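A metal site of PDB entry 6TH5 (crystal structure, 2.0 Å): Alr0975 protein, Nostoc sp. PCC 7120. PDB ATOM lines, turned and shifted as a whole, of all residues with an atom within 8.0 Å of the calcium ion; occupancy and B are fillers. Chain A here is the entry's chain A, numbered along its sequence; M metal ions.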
ATOM      1  N   ARG A  27     -20.164  -9.927 -30.137  1.00  0.00           N
ATOM      2  CA  ARG A  27     -21.329  -9.716 -30.974  1.00  0.00           C
ATOM      3  C   ARG A  27     -21.804 -10.982 -31.667  1.00  0.00           C
ATOM      4  O   ARG A  27     -22.507 -10.904 -32.682  1.00  0.00           O
ATOM      5  CB  ARG A  27     -21.034  -8.654 -32.036  1.00  0.00           C
ATOM      6  CG  ARG A  27     -19.834  -9.002 -32.920  1.00  0.00           C
ATOM      7  CD  ARG A  27     -19.717  -8.065 -34.130  1.00  0.00           C
ATOM      8  NE  ARG A  27     -18.733  -8.571 -35.093  1.00  0.00           N
ATOM      9  CZ  ARG A  27     -17.896  -7.807 -35.781  1.00  0.00           C
ATOM     10  NH1 ARG A  27     -17.032  -8.377 -36.619  1.00  0.00           N
ATOM     11  NH2 ARG A  27     -17.913  -6.483 -35.658  1.00  0.00           N
ATOM     12  N   GLU A  28     -21.451 -12.165 -31.142  1.00  0.00           N
ATOM     13  CA  GLU A  28     -21.875 -13.400 -31.788  1.00  0.00           C
ATOM     14  C   GLU A  28     -23.396 -13.487 -31.871  1.00  0.00           C
ATOM     15  O   GLU A  28     -23.946 -14.022 -32.849  1.00  0.00           O
ATOM     16  CB  GLU A  28     -21.331 -14.611 -31.023  1.00  0.00           C
ATOM     17  CG  GLU A  28     -19.826 -14.771 -31.085  1.00  0.00           C
ATOM     18  CD  GLU A  28     -19.313 -14.841 -32.500  1.00  0.00           C
ATOM     19  OE1 GLU A  28     -19.839 -15.661 -33.298  1.00  0.00           O
ATOM     20  OE2 GLU A  28     -18.389 -14.071 -32.822  1.00  0.00           O
ATOM     21  N   ASP A  29     -24.089 -12.987 -30.860  1.00  0.00           N
ATOM     22  CA  ASP A  29     -25.525 -13.177 -30.768  1.00  0.00           C
ATOM     23  C   ASP A  29     -26.325 -12.215 -31.640  1.00  0.00           C
ATOM     24  O   ASP A  29     -27.499 -12.467 -31.883  1.00  0.00           O
ATOM     25  CB  ASP A  29     -25.975 -13.023 -29.299  1.00  0.00           C
ATOM     26  CG  ASP A  29     -25.453 -14.144 -28.410  1.00  0.00           C
ATOM     27  OD1 ASP A  29     -24.741 -15.025 -28.920  1.00  0.00           O
ATOM     28  OD2 ASP A  29     -25.785 -14.130 -27.207  1.00  0.00           O
ATOM     29  N   PHE A  30     -25.711 -11.138 -32.120  1.00  0.00           N
ATOM     30  CA  PHE A  30     -26.465 -10.139 -32.878  1.00  0.00           C
ATOM     31  C   PHE A  30     -27.042 -10.746 -34.149  1.00  0.00           C
ATOM     32  O   PHE A  30     -28.234 -10.595 -34.432  1.00  0.00           O
ATOM     33  CB  PHE A  30     -25.571  -8.949 -33.231  1.00  0.00           C
ATOM     34  CG  PHE A  30     -26.175  -8.047 -34.275  1.00  0.00           C
ATOM     35  CD1 PHE A  30     -27.045  -7.038 -33.919  1.00  0.00           C
ATOM     36  CD2 PHE A  30     -25.872  -8.224 -35.621  1.00  0.00           C
ATOM     37  CE1 PHE A  30     -27.608  -6.217 -34.881  1.00  0.00           C
ATOM     38  CE2 PHE A  30     -26.444  -7.413 -36.586  1.00  0.00           C
ATOM     39  CZ  PHE A  30     -27.302  -6.401 -36.209  1.00  0.00           C
ATOM     40  N   PRO A  32     -27.789 -13.918 -35.332  1.00  0.00           N
ATOM     41  CA  PRO A  32     -28.994 -14.757 -35.197  1.00  0.00           C
ATOM     42  C   PRO A  32     -30.193 -13.986 -34.641  1.00  0.00           C
ATOM     43  O   PRO A  32     -31.336 -14.227 -35.069  1.00  0.00           O
ATOM     44  CB  PRO A  32     -28.547 -15.886 -34.257  1.00  0.00           C
ATOM     45  CG  PRO A  32     -27.287 -15.421 -33.623  1.00  0.00           C
ATOM     46  CD  PRO A  32     -26.629 -14.492 -34.620  1.00  0.00           C
ATOM     47  N   LEU A  33     -29.954 -13.062 -33.705  1.00  0.00           N
ATOM     48  CA  LEU A  33     -31.065 -12.320 -33.130  1.00  0.00           C
ATOM     49  C   LEU A  33     -31.658 -11.341 -34.147  1.00  0.00           C
ATOM     50  O   LEU A  33     -32.873 -11.160 -34.210  1.00  0.00           O
ATOM     51  CB  LEU A  33     -30.612 -11.582 -31.876  1.00  0.00           C
ATOM     52  CG  LEU A  33     -30.422 -12.451 -30.635  1.00  0.00           C
ATOM     53  CD1 LEU A  33     -29.790 -11.639 -29.511  1.00  0.00           C
ATOM     54  CD2 LEU A  33     -31.733 -13.076 -30.197  1.00  0.00           C
ATOM     55  N   LEU A  58     -32.075 -20.377 -31.217  1.00  0.00           N
ATOM     56  CA  LEU A  58     -31.511 -21.632 -30.742  1.00  0.00           C
ATOM     57  C   LEU A  58     -31.933 -22.827 -31.601  1.00  0.00           C
ATOM     58  O   LEU A  58     -31.427 -23.937 -31.375  1.00  0.00           O
ATOM     59  CB  LEU A  58     -31.908 -21.886 -29.295  1.00  0.00           C
ATOM     60  CG  LEU A  58     -31.196 -21.048 -28.239  1.00  0.00           C
ATOM     61  CD1 LEU A  58     -31.906 -21.190 -26.894  1.00  0.00           C
ATOM     62  CD2 LEU A  58     -29.738 -21.443 -28.133  1.00  0.00           C
ATOM     63  N   GLN A 131     -20.291 -11.966 -16.960  1.00  0.00           N
ATOM     64  CA  GLN A 131     -20.982 -13.155 -17.449  1.00  0.00           C
ATOM     65  C   GLN A 131     -21.723 -12.891 -18.755  1.00  0.00           C
ATOM     66  O   GLN A 131     -21.798 -13.772 -19.614  1.00  0.00           O
ATOM     67  CB  GLN A 131     -21.943 -13.674 -16.379  1.00  0.00           C
ATOM     68  CG  GLN A 131     -21.255 -14.222 -15.139  1.00  0.00           C
ATOM     69  CD  GLN A 131     -22.172 -14.302 -13.932  1.00  0.00           C
ATOM     70  OE1 GLN A 131     -21.738 -14.092 -12.799  1.00  0.00           O
ATOM     71  NE2 GLN A 131     -23.442 -14.589 -14.173  1.00  0.00           N
ATOM     72  N   VAL A 132     -22.296 -11.699 -18.906  1.00  0.00           N
ATOM     73  CA  VAL A 132     -23.026 -11.389 -20.132  1.00  0.00           C
ATOM     74  C   VAL A 132     -22.052 -11.190 -21.292  1.00  0.00           C
ATOM     75  O   VAL A 132     -22.262 -11.701 -22.391  1.00  0.00           O
ATOM     76  CB  VAL A 132     -23.918 -10.148 -19.933  1.00  0.00           C
ATOM     77  CG1 VAL A 132     -24.542  -9.733 -21.255  1.00  0.00           C
ATOM     78  CG2 VAL A 132     -25.003 -10.421 -18.892  1.00  0.00           C
ATOM     79  N   ALA A 133     -20.979 -10.441 -21.051  1.00  0.00           N
ATOM     80  CA  ALA A 133     -20.004 -10.187 -22.104  1.00  0.00           C
ATOM     81  C   ALA A 133     -19.474 -11.496 -22.681  1.00  0.00           C
ATOM     82  O   ALA A 133     -19.241 -11.595 -23.890  1.00  0.00           O
ATOM     83  CB  ALA A 133     -18.858  -9.336 -21.577  1.00  0.00           C
ATOM     84  N   GLU A 134     -19.289 -12.510 -21.839  1.00  0.00           N
ATOM     85  CA  GLU A 134     -18.805 -13.796 -22.325  1.00  0.00           C
ATOM     86  C   GLU A 134     -19.879 -14.514 -23.137  1.00  0.00           C
ATOM     87  O   GLU A 134     -19.597 -15.079 -24.194  1.00  0.00           O
ATOM     88  CB  GLU A 134     -18.337 -14.665 -21.160  1.00  0.00           C
ATOM     89  CG  GLU A 134     -17.399 -15.803 -21.553  1.00  0.00           C
ATOM     90  CD  GLU A 134     -16.268 -15.371 -22.489  1.00  0.00           C
ATOM     91  OE1 GLU A 134     -15.627 -14.318 -22.216  1.00  0.00           O
ATOM     92  OE2 GLU A 134     -16.042 -16.068 -23.500  1.00  0.00           O
ATOM     93  N   ASN A 135     -21.125 -14.500 -22.653  1.00  0.00           N
ATOM     94  CA  ASN A 135     -22.214 -15.098 -23.418  1.00  0.00           C
ATOM     95  C   ASN A 135     -22.310 -14.463 -24.806  1.00  0.00           C
ATOM     96  O   ASN A 135     -22.469 -15.167 -25.813  1.00  0.00           O
ATOM     97  CB  ASN A 135     -23.541 -14.935 -22.681  1.00  0.00           C
ATOM     98  CG  ASN A 135     -24.713 -15.610 -23.387  1.00  0.00           C
ATOM     99  OD1 ASN A 135     -25.045 -15.262 -24.532  1.00  0.00           O
ATOM    100  ND2 ASN A 135     -25.329 -16.566 -22.720  1.00  0.00           N
ATOM    101  N   LEU A 136     -22.204 -13.136 -24.874  1.00  0.00           N
ATOM    102  CA  LEU A 136     -22.279 -12.442 -26.157  1.00  0.00           C
ATOM    103  C   LEU A 136     -21.107 -12.761 -27.068  1.00  0.00           C
ATOM    104  O   LEU A 136     -21.100 -12.297 -28.212  1.00  0.00           O
ATOM    105  CB  LEU A 136     -22.376 -10.935 -25.919  1.00  0.00           C
ATOM    106  CG  LEU A 136     -23.595 -10.503 -25.088  1.00  0.00           C
ATOM    107  CD1 LEU A 136     -23.572  -9.012 -24.800  1.00  0.00           C
ATOM    108  CD2 LEU A 136     -24.895 -10.881 -25.791  1.00  0.00           C
ATOM    109  N   LYS A 137     -20.123 -13.523 -26.592  1.00  0.00           N
ATOM    110  CA  LYS A 137     -19.003 -13.970 -27.414  1.00  0.00           C
ATOM    111  C   LYS A 137     -19.147 -15.398 -27.897  1.00  0.00           C
ATOM    112  O   LYS A 137     -18.276 -15.880 -28.627  1.00  0.00           O
ATOM    113  CB  LYS A 137     -17.686 -13.837 -26.634  1.00  0.00           C
ATOM    114  CG  LYS A 137     -17.194 -12.412 -26.446  1.00  0.00           C
ATOM    115  CD  LYS A 137     -15.717 -12.406 -26.008  1.00  0.00           C
ATOM    116  CE  LYS A 137     -15.268 -11.039 -25.522  1.00  0.00           C
ATOM    117  NZ  LYS A 137     -16.002 -10.596 -24.298  1.00  0.00           N
ATOM    118  N   GLN A 138     -20.228 -16.094 -27.512  1.00  0.00           N
ATOM    119  CA  GLN A 138     -20.417 -17.488 -27.877  1.00  0.00           C
ATOM    120  C   GLN A 138     -21.785 -17.711 -28.499  1.00  0.00           C
ATOM    121  O   GLN A 138     -22.763 -17.048 -28.149  1.00  0.00           O
ATOM    122  CB  GLN A 138     -20.288 -18.423 -26.650  1.00  0.00           C
ATOM    123  CG  GLN A 138     -19.417 -17.898 -25.522  1.00  0.00           C
ATOM    124  CD  GLN A 138     -19.276 -18.903 -24.388  1.00  0.00           C
ATOM    125  OE1 GLN A 138     -18.636 -19.936 -24.534  1.00  0.00           O
ATOM    126  NE2 GLN A 138     -19.885 -18.595 -23.247  1.00  0.00           N
ATOM    127  N   ASP A 139     -21.844 -18.672 -29.425  1.00  0.00           N
ATOM    128  CA  ASP A 139     -23.094 -19.103 -30.004  1.00  0.00           C
ATOM    129  C   ASP A 139     -23.765 -20.129 -29.095  1.00  0.00           C
ATOM    130  O   ASP A 139     -23.195 -20.611 -28.114  1.00  0.00           O
ATOM    131  CB  ASP A 139     -22.870 -19.703 -31.400  1.00  0.00           C
ATOM    132  CG  ASP A 139     -22.137 -18.751 -32.324  1.00  0.00           C
ATOM    133  OD1 ASP A 139     -22.602 -17.611 -32.502  1.00  0.00           O
ATOM    134  OD2 ASP A 139     -21.088 -19.160 -32.883  1.00  0.00           O
ATOM    135  N   GLY A 140     -25.005 -20.479 -29.441  1.00  0.00           N
ATOM    136  CA  GLY A 140     -25.726 -21.497 -28.705  1.00  0.00           C
ATOM    137  C   GLY A 140     -26.287 -21.051 -27.378  1.00  0.00           C
ATOM    138  O   GLY A 140     -26.822 -21.902 -26.652  1.00  0.00           O
ATOM    139  N   ASN A 141     -26.196 -19.767 -27.039  1.00  0.00           N
ATOM    140  CA  ASN A 141     -26.781 -19.239 -25.818  1.00  0.00           C
ATOM    141  C   ASN A 141     -27.078 -17.768 -26.017  1.00  0.00           C
ATOM    142  O   ASN A 141     -26.475 -17.093 -26.852  1.00  0.00           O
ATOM    143  CB  ASN A 141     -25.854 -19.453 -24.609  1.00  0.00           C
ATOM    144  CG  ASN A 141     -24.437 -18.995 -24.867  1.00  0.00           C
ATOM    145  OD1 ASN A 141     -24.218 -17.973 -25.522  1.00  0.00           O
ATOM    146  ND2 ASN A 141     -23.474 -19.733 -24.347  1.00  0.00           N
ATOM    147  N   PHE A 142     -28.018 -17.256 -25.221  1.00  0.00           N
ATOM    148  CA  PHE A 142     -28.499 -15.891 -25.398  1.00  0.00           C
ATOM    149  C   PHE A 142     -28.858 -15.300 -24.048  1.00  0.00           C
ATOM    150  O   PHE A 142     -29.054 -16.007 -23.062  1.00  0.00           O
ATOM    151  CB  PHE A 142     -29.687 -15.854 -26.350  1.00  0.00           C
ATOM    152  CG  PHE A 142     -29.362 -16.317 -27.732  1.00  0.00           C
ATOM    153  CD1 PHE A 142     -28.867 -15.425 -28.685  1.00  0.00           C
ATOM    154  CD2 PHE A 142     -29.520 -17.646 -28.089  1.00  0.00           C
ATOM    155  CE1 PHE A 142     -28.544 -15.860 -29.948  1.00  0.00           C
ATOM    156  CE2 PHE A 142     -29.199 -18.077 -29.361  1.00  0.00           C
ATOM    157  CZ  PHE A 142     -28.702 -17.183 -30.291  1.00  0.00           C
ATOM    158  N   VAL A 143     -28.937 -13.968 -24.020  1.00  0.00           N
ATOM    159  CA  VAL A 143     -29.216 -13.203 -22.813  1.00  0.00           C
ATOM    160  C   VAL A 143     -30.486 -12.395 -23.031  1.00  0.00           C
ATOM    161  O   VAL A 143     -30.641 -11.752 -24.071  1.00  0.00           O
ATOM    162  CB  VAL A 143     -28.048 -12.272 -22.454  1.00  0.00           C
ATOM    163  CG1 VAL A 143     -28.259 -11.646 -21.093  1.00  0.00           C
ATOM    164  CG2 VAL A 143     -26.713 -13.022 -22.527  1.00  0.00           C
ATOM    165  N   LEU A 163     -30.347  -9.053 -25.360  1.00  0.00           N
ATOM    166  CA  LEU A 163     -29.103  -8.336 -25.611  1.00  0.00           C
ATOM    167  C   LEU A 163     -28.428  -8.966 -26.820  1.00  0.00           C
ATOM    168  O   LEU A 163     -28.450 -10.195 -26.977  1.00  0.00           O
ATOM    169  CB  LEU A 163     -28.164  -8.381 -24.416  1.00  0.00           C
ATOM    170  CG  LEU A 163     -28.647  -7.742 -23.116  1.00  0.00           C
ATOM    171  CD1 LEU A 163     -27.556  -7.854 -22.035  1.00  0.00           C
ATOM    172  CD2 LEU A 163     -29.041  -6.302 -23.321  1.00  0.00           C
ATOM    173  N   ALA A 164     -27.833  -8.125 -27.668  1.00  0.00           N
ATOM    174  CA  ALA A 164     -27.188  -8.580 -28.892  1.00  0.00           C
ATOM    175  C   ALA A 164     -25.671  -8.497 -28.853  1.00  0.00           C
ATOM    176  O   ALA A 164     -24.995  -9.374 -29.410  1.00  0.00           O
ATOM    177  CB  ALA A 164     -27.709  -7.781 -30.085  1.00  0.00           C
ATOM    178  N   PHE A 212     -30.153 -16.285 -18.650  1.00  0.00           N
ATOM    179  CA  PHE A 212     -29.339 -16.960 -19.649  1.00  0.00           C
ATOM    180  C   PHE A 212     -30.135 -18.125 -20.231  1.00  0.00           C
ATOM    181  O   PHE A 212     -30.753 -18.893 -19.493  1.00  0.00           O
ATOM    182  CB  PHE A 212     -28.035 -17.477 -19.035  1.00  0.00           C
ATOM    183  CG  PHE A 212     -27.058 -16.379 -18.691  1.00  0.00           C
ATOM    184  CD1 PHE A 212     -26.580 -15.515 -19.662  1.00  0.00           C
ATOM    185  CD2 PHE A 212     -26.631 -16.215 -17.390  1.00  0.00           C
ATOM    186  CE1 PHE A 212     -25.702 -14.524 -19.353  1.00  0.00           C
ATOM    187  CE2 PHE A 212     -25.732 -15.209 -17.057  1.00  0.00           C
ATOM    188  CZ  PHE A 212     -25.263 -14.361 -18.043  1.00  0.00           C
ATOM    189  N   VAL A 213     -30.100 -18.268 -21.555  1.00  0.00           N
ATOM    190  CA  VAL A 213     -30.868 -19.297 -22.252  1.00  0.00           C
ATOM    191  C   VAL A 213     -29.915 -20.112 -23.100  1.00  0.00           C
ATOM    192  O   VAL A 213     -29.057 -19.546 -23.801  1.00  0.00           O
ATOM    193  CB  VAL A 213     -31.988 -18.680 -23.117  1.00  0.00           C
ATOM    194  CG1 VAL A 213     -32.984 -19.758 -23.516  1.00  0.00           C
ATOM    195  CG2 VAL A 213     -32.678 -17.543 -22.374  1.00  0.00           C
HETATM  196 CA    CA M   1     -24.419 -16.017 -26.752  1.00  0.00          CA
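The calcium ion is bound by OD1 of Asn 141, O of Asn 141, O of Asn 135, OD2 of Asp 29, O of Gln 138, OD1 of Asp 29 and OD1 of Asn 135. The calcium ion has seven donor atoms within binding distance.
Four residues have an atom within 4 Å of the calcium ion: Asp 29, Asn 135, Gln 138 and Asn 141.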
